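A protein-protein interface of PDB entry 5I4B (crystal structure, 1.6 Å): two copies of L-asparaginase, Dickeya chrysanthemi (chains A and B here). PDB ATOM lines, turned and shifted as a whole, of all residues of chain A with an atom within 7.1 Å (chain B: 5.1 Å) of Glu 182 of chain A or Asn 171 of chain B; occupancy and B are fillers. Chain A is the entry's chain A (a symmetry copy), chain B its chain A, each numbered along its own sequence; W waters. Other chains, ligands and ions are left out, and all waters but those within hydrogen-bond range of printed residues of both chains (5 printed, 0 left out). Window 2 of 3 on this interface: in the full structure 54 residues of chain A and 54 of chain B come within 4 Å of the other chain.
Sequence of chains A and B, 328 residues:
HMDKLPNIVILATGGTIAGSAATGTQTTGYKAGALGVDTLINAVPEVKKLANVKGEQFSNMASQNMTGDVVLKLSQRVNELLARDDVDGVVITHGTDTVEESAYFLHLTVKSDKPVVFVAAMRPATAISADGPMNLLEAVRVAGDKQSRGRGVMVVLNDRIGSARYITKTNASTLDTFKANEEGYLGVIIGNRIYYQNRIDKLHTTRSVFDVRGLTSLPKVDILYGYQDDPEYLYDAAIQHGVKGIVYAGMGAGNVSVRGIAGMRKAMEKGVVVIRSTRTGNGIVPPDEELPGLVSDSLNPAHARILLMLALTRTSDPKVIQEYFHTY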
ATOM      1  N   TYR A 166      10.112 -11.283  16.113  1.00  0.00           N
ATOM      2  CA  TYR A 166       8.776 -10.616  16.081  1.00  0.00           C
ATOM      3  C   TYR A 166       8.817  -9.132  15.685  1.00  0.00           C
ATOM      4  O   TYR A 166       7.841  -8.616  15.144  1.00  0.00           O
ATOM      5  CB  TYR A 166       8.091 -10.814  17.405  1.00  0.00           C
ATOM      6  CG  TYR A 166       7.838 -12.267  17.792  1.00  0.00           C
ATOM      7  CD1 TYR A 166       7.438 -13.196  16.852  1.00  0.00           C
ATOM      8  CD2 TYR A 166       7.887 -12.648  19.123  1.00  0.00           C
ATOM      9  CE1 TYR A 166       7.082 -14.505  17.241  1.00  0.00           C
ATOM     10  CE2 TYR A 166       7.557 -13.914  19.530  1.00  0.00           C
ATOM     11  CZ  TYR A 166       7.201 -14.868  18.553  1.00  0.00           C
ATOM     12  OH  TYR A 166       6.888 -16.182  18.942  1.00  0.00           O
ATOM     13  N   LYS A 179       7.570  -2.260  16.767  1.00  0.00           N
ATOM     14  CA  LYS A 179       6.508  -2.912  17.557  1.00  0.00           C
ATOM     15  C   LYS A 179       6.334  -4.345  17.041  1.00  0.00           C
ATOM     16  O   LYS A 179       6.678  -4.624  15.921  1.00  0.00           O
ATOM     17  CB  LYS A 179       5.182  -2.181  17.331  1.00  0.00           C
ATOM     18  CG  LYS A 179       5.156  -0.683  17.572  1.00  0.00           C
ATOM     19  CD  LYS A 179       3.749  -0.119  17.276  1.00  0.00           C
ATOM     20  CE  LYS A 179       3.793   1.415  17.128  1.00  0.00           C
ATOM     21  NZ  LYS A 179       4.074   2.071  18.452  1.00  0.00           N
ATOM     22  N   ALA A 180       5.738  -5.214  17.857  1.00  0.00           N
ATOM     23  CA  ALA A 180       5.285  -6.518  17.448  1.00  0.00           C
ATOM     24  C   ALA A 180       3.822  -6.551  17.906  1.00  0.00           C
ATOM     25  O   ALA A 180       3.535  -6.883  19.076  1.00  0.00           O
ATOM     26  CB  ALA A 180       6.129  -7.585  18.149  1.00  0.00           C
ATOM     27  N   ASN A 181       2.903  -6.204  17.035  1.00  0.00           N
ATOM     28  CA  ASN A 181       1.548  -5.953  17.514  1.00  0.00           C
ATOM     29  C   ASN A 181       0.950  -7.186  18.206  1.00  0.00           C
ATOM     30  O   ASN A 181       0.293  -7.038  19.251  1.00  0.00           O
ATOM     31  CB  ASN A 181       0.652  -5.489  16.423  1.00  0.00           C
ATOM     32  CG  ASN A 181       1.093  -4.119  15.856  1.00  0.00           C
ATOM     33  OD1 ASN A 181       1.176  -3.135  16.570  1.00  0.00           O
ATOM     34  ND2 ASN A 181       1.351  -4.062  14.552  1.00  0.00           N
ATOM     35  N   GLU A 182       1.177  -8.376  17.672  1.00  0.00           N
ATOM     36  CA  GLU A 182       0.515  -9.547  18.231  1.00  0.00           C
ATOM     37  C   GLU A 182       1.357 -10.225  19.355  1.00  0.00           C
ATOM     38  O   GLU A 182       0.794 -10.990  20.151  1.00  0.00           O
ATOM     39  CB  GLU A 182       0.202 -10.528  17.160  1.00  0.00           C
ATOM     40  CG  GLU A 182      -0.827  -9.984  16.119  1.00  0.00           C
ATOM     41  CD  GLU A 182      -2.251 -10.018  16.662  1.00  0.00           C
ATOM     42  OE1 GLU A 182      -2.714 -11.098  17.116  1.00  0.00           O
ATOM     43  OE2 GLU A 182      -2.916  -8.971  16.639  1.00  0.00           O
ATOM     44  N   GLU A 183       2.662 -10.015  19.341  1.00  0.00           N
ATOM     45  CA  GLU A 183       3.550 -10.723  20.203  1.00  0.00           C
ATOM     46  C   GLU A 183       4.184  -9.854  21.296  1.00  0.00           C
ATOM     47  O   GLU A 183       4.780 -10.431  22.252  1.00  0.00           O
ATOM     48  CB  GLU A 183       4.699 -11.349  19.402  1.00  0.00           C
ATOM     49  CG  GLU A 183       4.323 -12.181  18.258  1.00  0.00           C
ATOM     50  CD  GLU A 183       4.185 -11.445  16.953  1.00  0.00           C
ATOM     51  OE1 GLU A 183       4.222 -10.196  16.902  1.00  0.00           O
ATOM     52  OE2 GLU A 183       4.032 -12.189  15.936  1.00  0.00           O
ATOM     53  N   GLY A 184       4.048  -8.525  21.219  1.00  0.00           N
ATOM     54  CA  GLY A 184       4.545  -7.652  22.271  1.00  0.00           C
ATOM     55  C   GLY A 184       6.035  -7.602  22.379  1.00  0.00           C
ATOM     56  O   GLY A 184       6.753  -8.112  21.512  1.00  0.00           O
ATOM     57  N   GLY A 252      -3.899 -10.675   1.801  1.00  0.00           N
ATOM     58  CA  GLY A 252      -4.439 -11.358   2.923  1.00  0.00           C
ATOM     59  C   GLY A 252      -3.545 -12.466   3.472  1.00  0.00           C
ATOM     60  O   GLY A 252      -2.356 -12.272   3.641  1.00  0.00           O
ATOM     61  N   ALA A 253      -4.120 -13.629   3.613  1.00  0.00           N
ATOM     62  CA  ALA A 253      -3.451 -14.779   4.216  1.00  0.00           C
ATOM     63  C   ALA A 253      -2.712 -15.555   3.131  1.00  0.00           C
ATOM     64  O   ALA A 253      -3.022 -16.718   2.886  1.00  0.00           O
ATOM     65  CB  ALA A 253      -4.471 -15.651   4.918  1.00  0.00           C
ATOM     66  N   THR A 278       2.563 -12.520   3.890  1.00  0.00           N
ATOM     67  CA  THR A 278       1.481 -11.574   3.750  1.00  0.00           C
ATOM     68  C   THR A 278       2.034 -10.172   3.700  1.00  0.00           C
ATOM     69  O   THR A 278       3.015  -9.839   4.375  1.00  0.00           O
ATOM     70  CB  THR A 278       0.492 -11.767   4.915  1.00  0.00           C
ATOM     71  OG1 THR A 278      -0.592 -10.817   4.838  1.00  0.00           O
ATOM     72  CG2 THR A 278       1.170 -11.628   6.276  1.00  0.00           C
ATOM     73  N   THR A 280       0.142  -7.813   4.794  1.00  0.00           N
ATOM     74  CA  THR A 280      -0.734  -7.079   5.714  1.00  0.00           C
ATOM     75  C   THR A 280       0.010  -6.439   6.872  1.00  0.00           C
ATOM     76  O   THR A 280      -0.410  -5.365   7.312  1.00  0.00           O
ATOM     77  CB  THR A 280      -1.838  -8.010   6.288  1.00  0.00           C
ATOM     78  OG1 THR A 280      -1.236  -9.090   7.003  1.00  0.00           O
ATOM     79  CG2 THR A 280      -2.771  -8.515   5.180  1.00  0.00           C
ATOM     80  N   GLY A 281       1.107  -7.082   7.334  1.00  0.00           N
ATOM     81  CA  GLY A 281       1.955  -6.610   8.401  1.00  0.00           C
ATOM     82  C   GLY A 281       1.963  -7.516   9.651  1.00  0.00           C
ATOM     83  O   GLY A 281       2.866  -7.397  10.464  1.00  0.00           O
ATOM     84  N   ASN A 282       0.983  -8.389   9.774  1.00  0.00           N
ATOM     85  CA  ASN A 282       0.861  -9.166  10.995  1.00  0.00           C
ATOM     86  C   ASN A 282       0.124 -10.486  10.721  1.00  0.00           C
ATOM     87  O   ASN A 282      -0.690 -10.552   9.824  1.00  0.00           O
ATOM     88  CB  ASN A 282       0.008  -8.407  12.051  1.00  0.00           C
ATOM     89  CG  ASN A 282       0.542  -7.008  12.396  1.00  0.00           C
ATOM     90  OD1 ASN A 282       1.289  -6.866  13.313  1.00  0.00           O
ATOM     91  ND2 ASN A 282       0.145  -5.985  11.642  1.00  0.00           N
ATOM     92  N   GLY A 283       0.329 -11.464  11.624  1.00  0.00           N
ATOM     93  CA  GLY A 283      -0.585 -12.619  11.718  1.00  0.00           C
ATOM     94  C   GLY A 283      -0.132 -13.859  10.944  1.00  0.00           C
ATOM     95  O   GLY A 283       0.983 -13.889  10.360  1.00  0.00           O
ATOM     96  N   ILE A 284      -0.995 -14.842  10.934  1.00  0.00           N
ATOM     97  CA  ILE A 284      -0.624 -16.192  10.508  1.00  0.00           C
ATOM     98  C   ILE A 284      -1.116 -16.450   9.094  1.00  0.00           C
ATOM     99  O   ILE A 284      -2.290 -16.247   8.788  1.00  0.00           O
ATOM    100  CB  ILE A 284      -1.313 -17.235  11.404  1.00  0.00           C
ATOM    101  CG1 ILE A 284      -0.784 -17.147  12.847  1.00  0.00           C
ATOM    102  CG2 ILE A 284      -1.192 -18.655  10.828  1.00  0.00           C
ATOM    103  CD1 ILE A 284       0.589 -17.656  13.037  1.00  0.00           C
ATOM    104  N   MET B 122     -14.271 -12.073   7.331  1.00  0.00           N
ATOM    105  CA  MET B 122     -13.075 -12.889   7.505  1.00  0.00           C
ATOM    106  C   MET B 122     -13.384 -14.386   7.672  1.00  0.00           C
ATOM    107  O   MET B 122     -12.471 -15.236   7.381  1.00  0.00           O
ATOM    108  CB  MET B 122     -12.229 -12.347   8.634  1.00  0.00           C
ATOM    109  CG  MET B 122     -11.516 -11.045   8.259  1.00  0.00           C
ATOM    110  SD  MET B 122     -10.236 -11.238   7.041  1.00  0.00           S
ATOM    111  CE  MET B 122      -8.941 -12.008   8.002  1.00  0.00           C
ATOM    112  N   LYS B 169      -6.130  -3.918   5.540  1.00  0.00           N
ATOM    113  CA  LYS B 169      -6.070  -5.214   6.173  1.00  0.00           C
ATOM    114  C   LYS B 169      -4.713  -5.385   6.821  1.00  0.00           C
ATOM    115  O   LYS B 169      -3.668  -5.473   6.127  1.00  0.00           O
ATOM    116  CB  LYS B 169      -6.308  -6.274   5.092  1.00  0.00           C
ATOM    117  CG  LYS B 169      -6.509  -7.666   5.691  1.00  0.00           C
ATOM    118  CD  LYS B 169      -6.971  -8.710   4.650  1.00  0.00           C
ATOM    119  CE  LYS B 169      -7.157 -10.093   5.326  1.00  0.00           C
ATOM    120  NZ  LYS B 169      -7.848 -11.061   4.427  1.00  0.00           N
ATOM    121  N   THR B 170      -4.656  -5.337   8.147  1.00  0.00           N
ATOM    122  CA  THR B 170      -3.403  -5.358   8.865  1.00  0.00           C
ATOM    123  C   THR B 170      -2.940  -6.721   9.299  1.00  0.00           C
ATOM    124  O   THR B 170      -1.808  -6.871   9.715  1.00  0.00           O
ATOM    125  CB  THR B 170      -3.407  -4.447  10.125  1.00  0.00           C
ATOM    126  OG1 THR B 170      -4.282  -4.968  11.149  1.00  0.00           O
ATOM    127  CG2 THR B 170      -3.795  -3.011   9.767  1.00  0.00           C
ATOM    128  N   ASN B 171      -3.845  -7.678   9.325  1.00  0.00           N
ATOM    129  CA  ASN B 171      -3.559  -9.018   9.823  1.00  0.00           C
ATOM    130  C   ASN B 171      -4.082 -10.004   8.772  1.00  0.00           C
ATOM    131  O   ASN B 171      -5.158  -9.882   8.204  1.00  0.00           O
ATOM    132  CB  ASN B 171      -4.230  -9.213  11.184  1.00  0.00           C
ATOM    133  CG  ASN B 171      -3.755 -10.508  11.874  1.00  0.00           C
ATOM    134  OD1 ASN B 171      -4.051 -11.631  11.383  1.00  0.00           O
ATOM    135  ND2 ASN B 171      -3.092 -10.362  13.017  1.00  0.00           N
ATOM    136  N   ALA B 172      -3.290 -11.038   8.515  1.00  0.00           N
ATOM    137  CA  ALA B 172      -3.683 -12.067   7.582  1.00  0.00           C
ATOM    138  C   ALA B 172      -5.018 -12.716   7.826  1.00  0.00           C
ATOM    139  O   ALA B 172      -5.722 -13.074   6.865  1.00  0.00           O
ATOM    140  CB  ALA B 172      -2.623 -13.157   7.558  1.00  0.00           C
ATOM    141  N   SER B 173      -5.387 -12.884   9.100  1.00  0.00           N
ATOM    142  CA  SER B 173      -6.389 -13.889   9.501  1.00  0.00           C
ATOM    143  C   SER B 173      -7.379 -13.586  10.600  1.00  0.00           C
ATOM    144  O   SER B 173      -8.274 -14.393  10.813  1.00  0.00           O
ATOM    145  CB  SER B 173      -5.673 -15.225   9.863  1.00  0.00           C
ATOM    146  OG  SER B 173      -4.935 -15.703   8.732  1.00  0.00           O
ATOM    147  N   THR B 174      -7.320 -12.419  11.204  1.00  0.00           N
ATOM    148  CA  THR B 174      -8.191 -12.105  12.363  1.00  0.00           C
ATOM    149  C   THR B 174      -9.428 -11.247  11.988  1.00  0.00           C
ATOM    150  O   THR B 174      -9.440 -10.547  10.992  1.00  0.00           O
ATOM    151  CB  THR B 174      -7.368 -11.299  13.379  1.00  0.00           C
ATOM    152  OG1 THR B 174      -6.799 -10.180  12.707  1.00  0.00           O
ATOM    153  CG2 THR B 174      -6.288 -12.174  13.963  1.00  0.00           C
ATOM    154  N   THR B 177      -8.878  -7.324  11.747  1.00  0.00           N
ATOM    155  CA  THR B 177      -7.797  -6.959  10.866  1.00  0.00           C
ATOM    156  C   THR B 177      -7.835  -5.551  10.282  1.00  0.00           C
ATOM    157  O   THR B 177      -6.766  -4.959  10.072  1.00  0.00           O
ATOM    158  CB  THR B 177      -7.710  -8.042   9.714  1.00  0.00           C
ATOM    159  OG1 THR B 177      -6.581  -7.764   8.892  1.00  0.00           O
ATOM    160  CG2 THR B 177      -8.974  -8.116   8.912  1.00  0.00           C
HETATM  161  O   HOH W   1      -1.482  -3.187   5.667  1.00  0.00           O
HETATM  162  O   HOH W   2      -2.415 -12.835  14.819  1.00  0.00           O
HETATM  163  O   HOH W   3      -2.644  -5.022  13.420  1.00  0.00           O
HETATM  164  O   HOH W   4      -3.071  -7.698  14.234  1.00  0.00           O
HETATM  165  O   HOH W   5      -3.340 -14.134  12.558  1.00  0.00           O
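Water W4 bridges the side-chain carboxylate of Glu 182 of chain A (2.7 Å) and the side-chain amide nitrogen of Asn 171 of chain B (2.9 Å).
Water W3 bridges the side-chain hydroxyl of Thr 170 of chain B and the side-chain amide nitrogen of Asn 282 of chain A.
Water W5 lies within hydrogen-bond range of the side-chain amide oxygen of Asn 171 of chain B (2.9 Å) and the backbone NH of Ile 284 of chain A (2.9 Å).
Water W2 lies within hydrogen-bond range of the side-chain carboxylate (OE1) of Glu 182 of chain A (2.9 Å) and the side-chain amide nitrogen (ND2) of Asn 171 of chain B (3.1 Å).
Water W1 bridges O of Thr 280 of chain A (2.9 Å) and O of Lys 169 of chain B (3.2 Å).
Ala 180 of chain A touches none of the printed residues of chain B.
Glu 182 of chain A touches just one residue of chain B: Asn 171.
Of the printed residues of chain B, Ala 253 of chain A touches Ala 172 and Ser 173.
Printed residues of chain A within 4 Å of Lys 169 of chain B: Gly 252 (3.7 Å) and Thr 280 (3.1 Å).
Asn 171 of chain B touches four residues of chain A.
Thr 174 of chain B touches none of the printed residues of chain A.
The nearest residue of chain A that does not touch Asn 171 of chain B is Ile 284 of chain A (4.5 Å).
Among the printed residues, pairs that only touch across the chains: Glu 182 of chain A with Asn 171 of chain B, Gly 252 of chain A with Lys 169 of chain B, Ala 253 of chain A with Ala 172 of chain B, Ala 253 of chain A with Ser 173 of chain B, Thr 280 of chain A with Asn 171 of chain B, Gly 281 of chain A with Thr 170 of chain B, Asn 282 of chain A with Asn 171 of chain B, Gly 283 of chain A with Asn 171 of chain B and Ile 284 of chain A with Ala 172 of chain B.
The backbone carbonyl oxygen (O) of Thr 280 of chain A sits close to the backbone carbonyl oxygen (O) of Lys 169 of chain B (3.5 Å).
The backbone carbonyl oxygen of Ile 284 of chain A lies within hydrogen-bond range of the side-chain hydroxyl of Ser 173 of chain B (2.7 Å).
The backbone carbonyl oxygen (O) of Thr 280 of chain A lies close to the backbone carbonyl oxygen (O) of Thr 170 of chain B (3.2 Å).
The backbone carbonyl oxygen (O) of Thr 170 of chain B sits at hydrogen-bond distance from the side-chain amide nitrogen (ND2) of Asn 282 of chain A, at 2.9 Å.
N of Ala 172 of chain B sits at hydrogen-bond distance from O of Asn 282 of chain A.
OG1 of Thr 280 of chain A sits at hydrogen-bond distance from N of Ala 172 of chain B (3.2 Å).
The side-chain amide oxygen (OD1) of Asn 171 of chain B lies within hydrogen-bond range of the backbone NH (N) of Ser 173 of chain B (2.9 Å).
OG1 of Thr 177 of chain B sits at hydrogen-bond distance from O of Asn 171 of chain B (2.6 Å).
N of Thr 174 of chain B is in hydrogen-bond range of OD1 of Asn 171 of chain B.
The side-chain amide nitrogen of Asn 181 of chain A is in hydrogen-bond range of the side-chain amide oxygen of Asn 282 of chain A.
The side-chain hydroxyl of Thr 278 of chain A lies within hydrogen-bond range of the backbone carbonyl oxygen of Gly 252 of chain A, 2.6 Å away.
OG1 of Thr 280 of chain A lies within hydrogen-bond range of O of Asn 282 of chain A (3.2 Å).
No position is printed for both chains.
Of the 15 pairs that touch across the chains among the printed residues, none has its exchanged pair printed and touching as well.
Hydrophobic or aromatic side chains of chain A within 4 Å of the printed part of chain B: Ala 253.
Of the 8 printed residues of chain B, 5 touch a printed residue of chain A.
Hydrophobic or aromatic side chains of chain B within 4 Å of the printed part of chain A: Ala 172.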
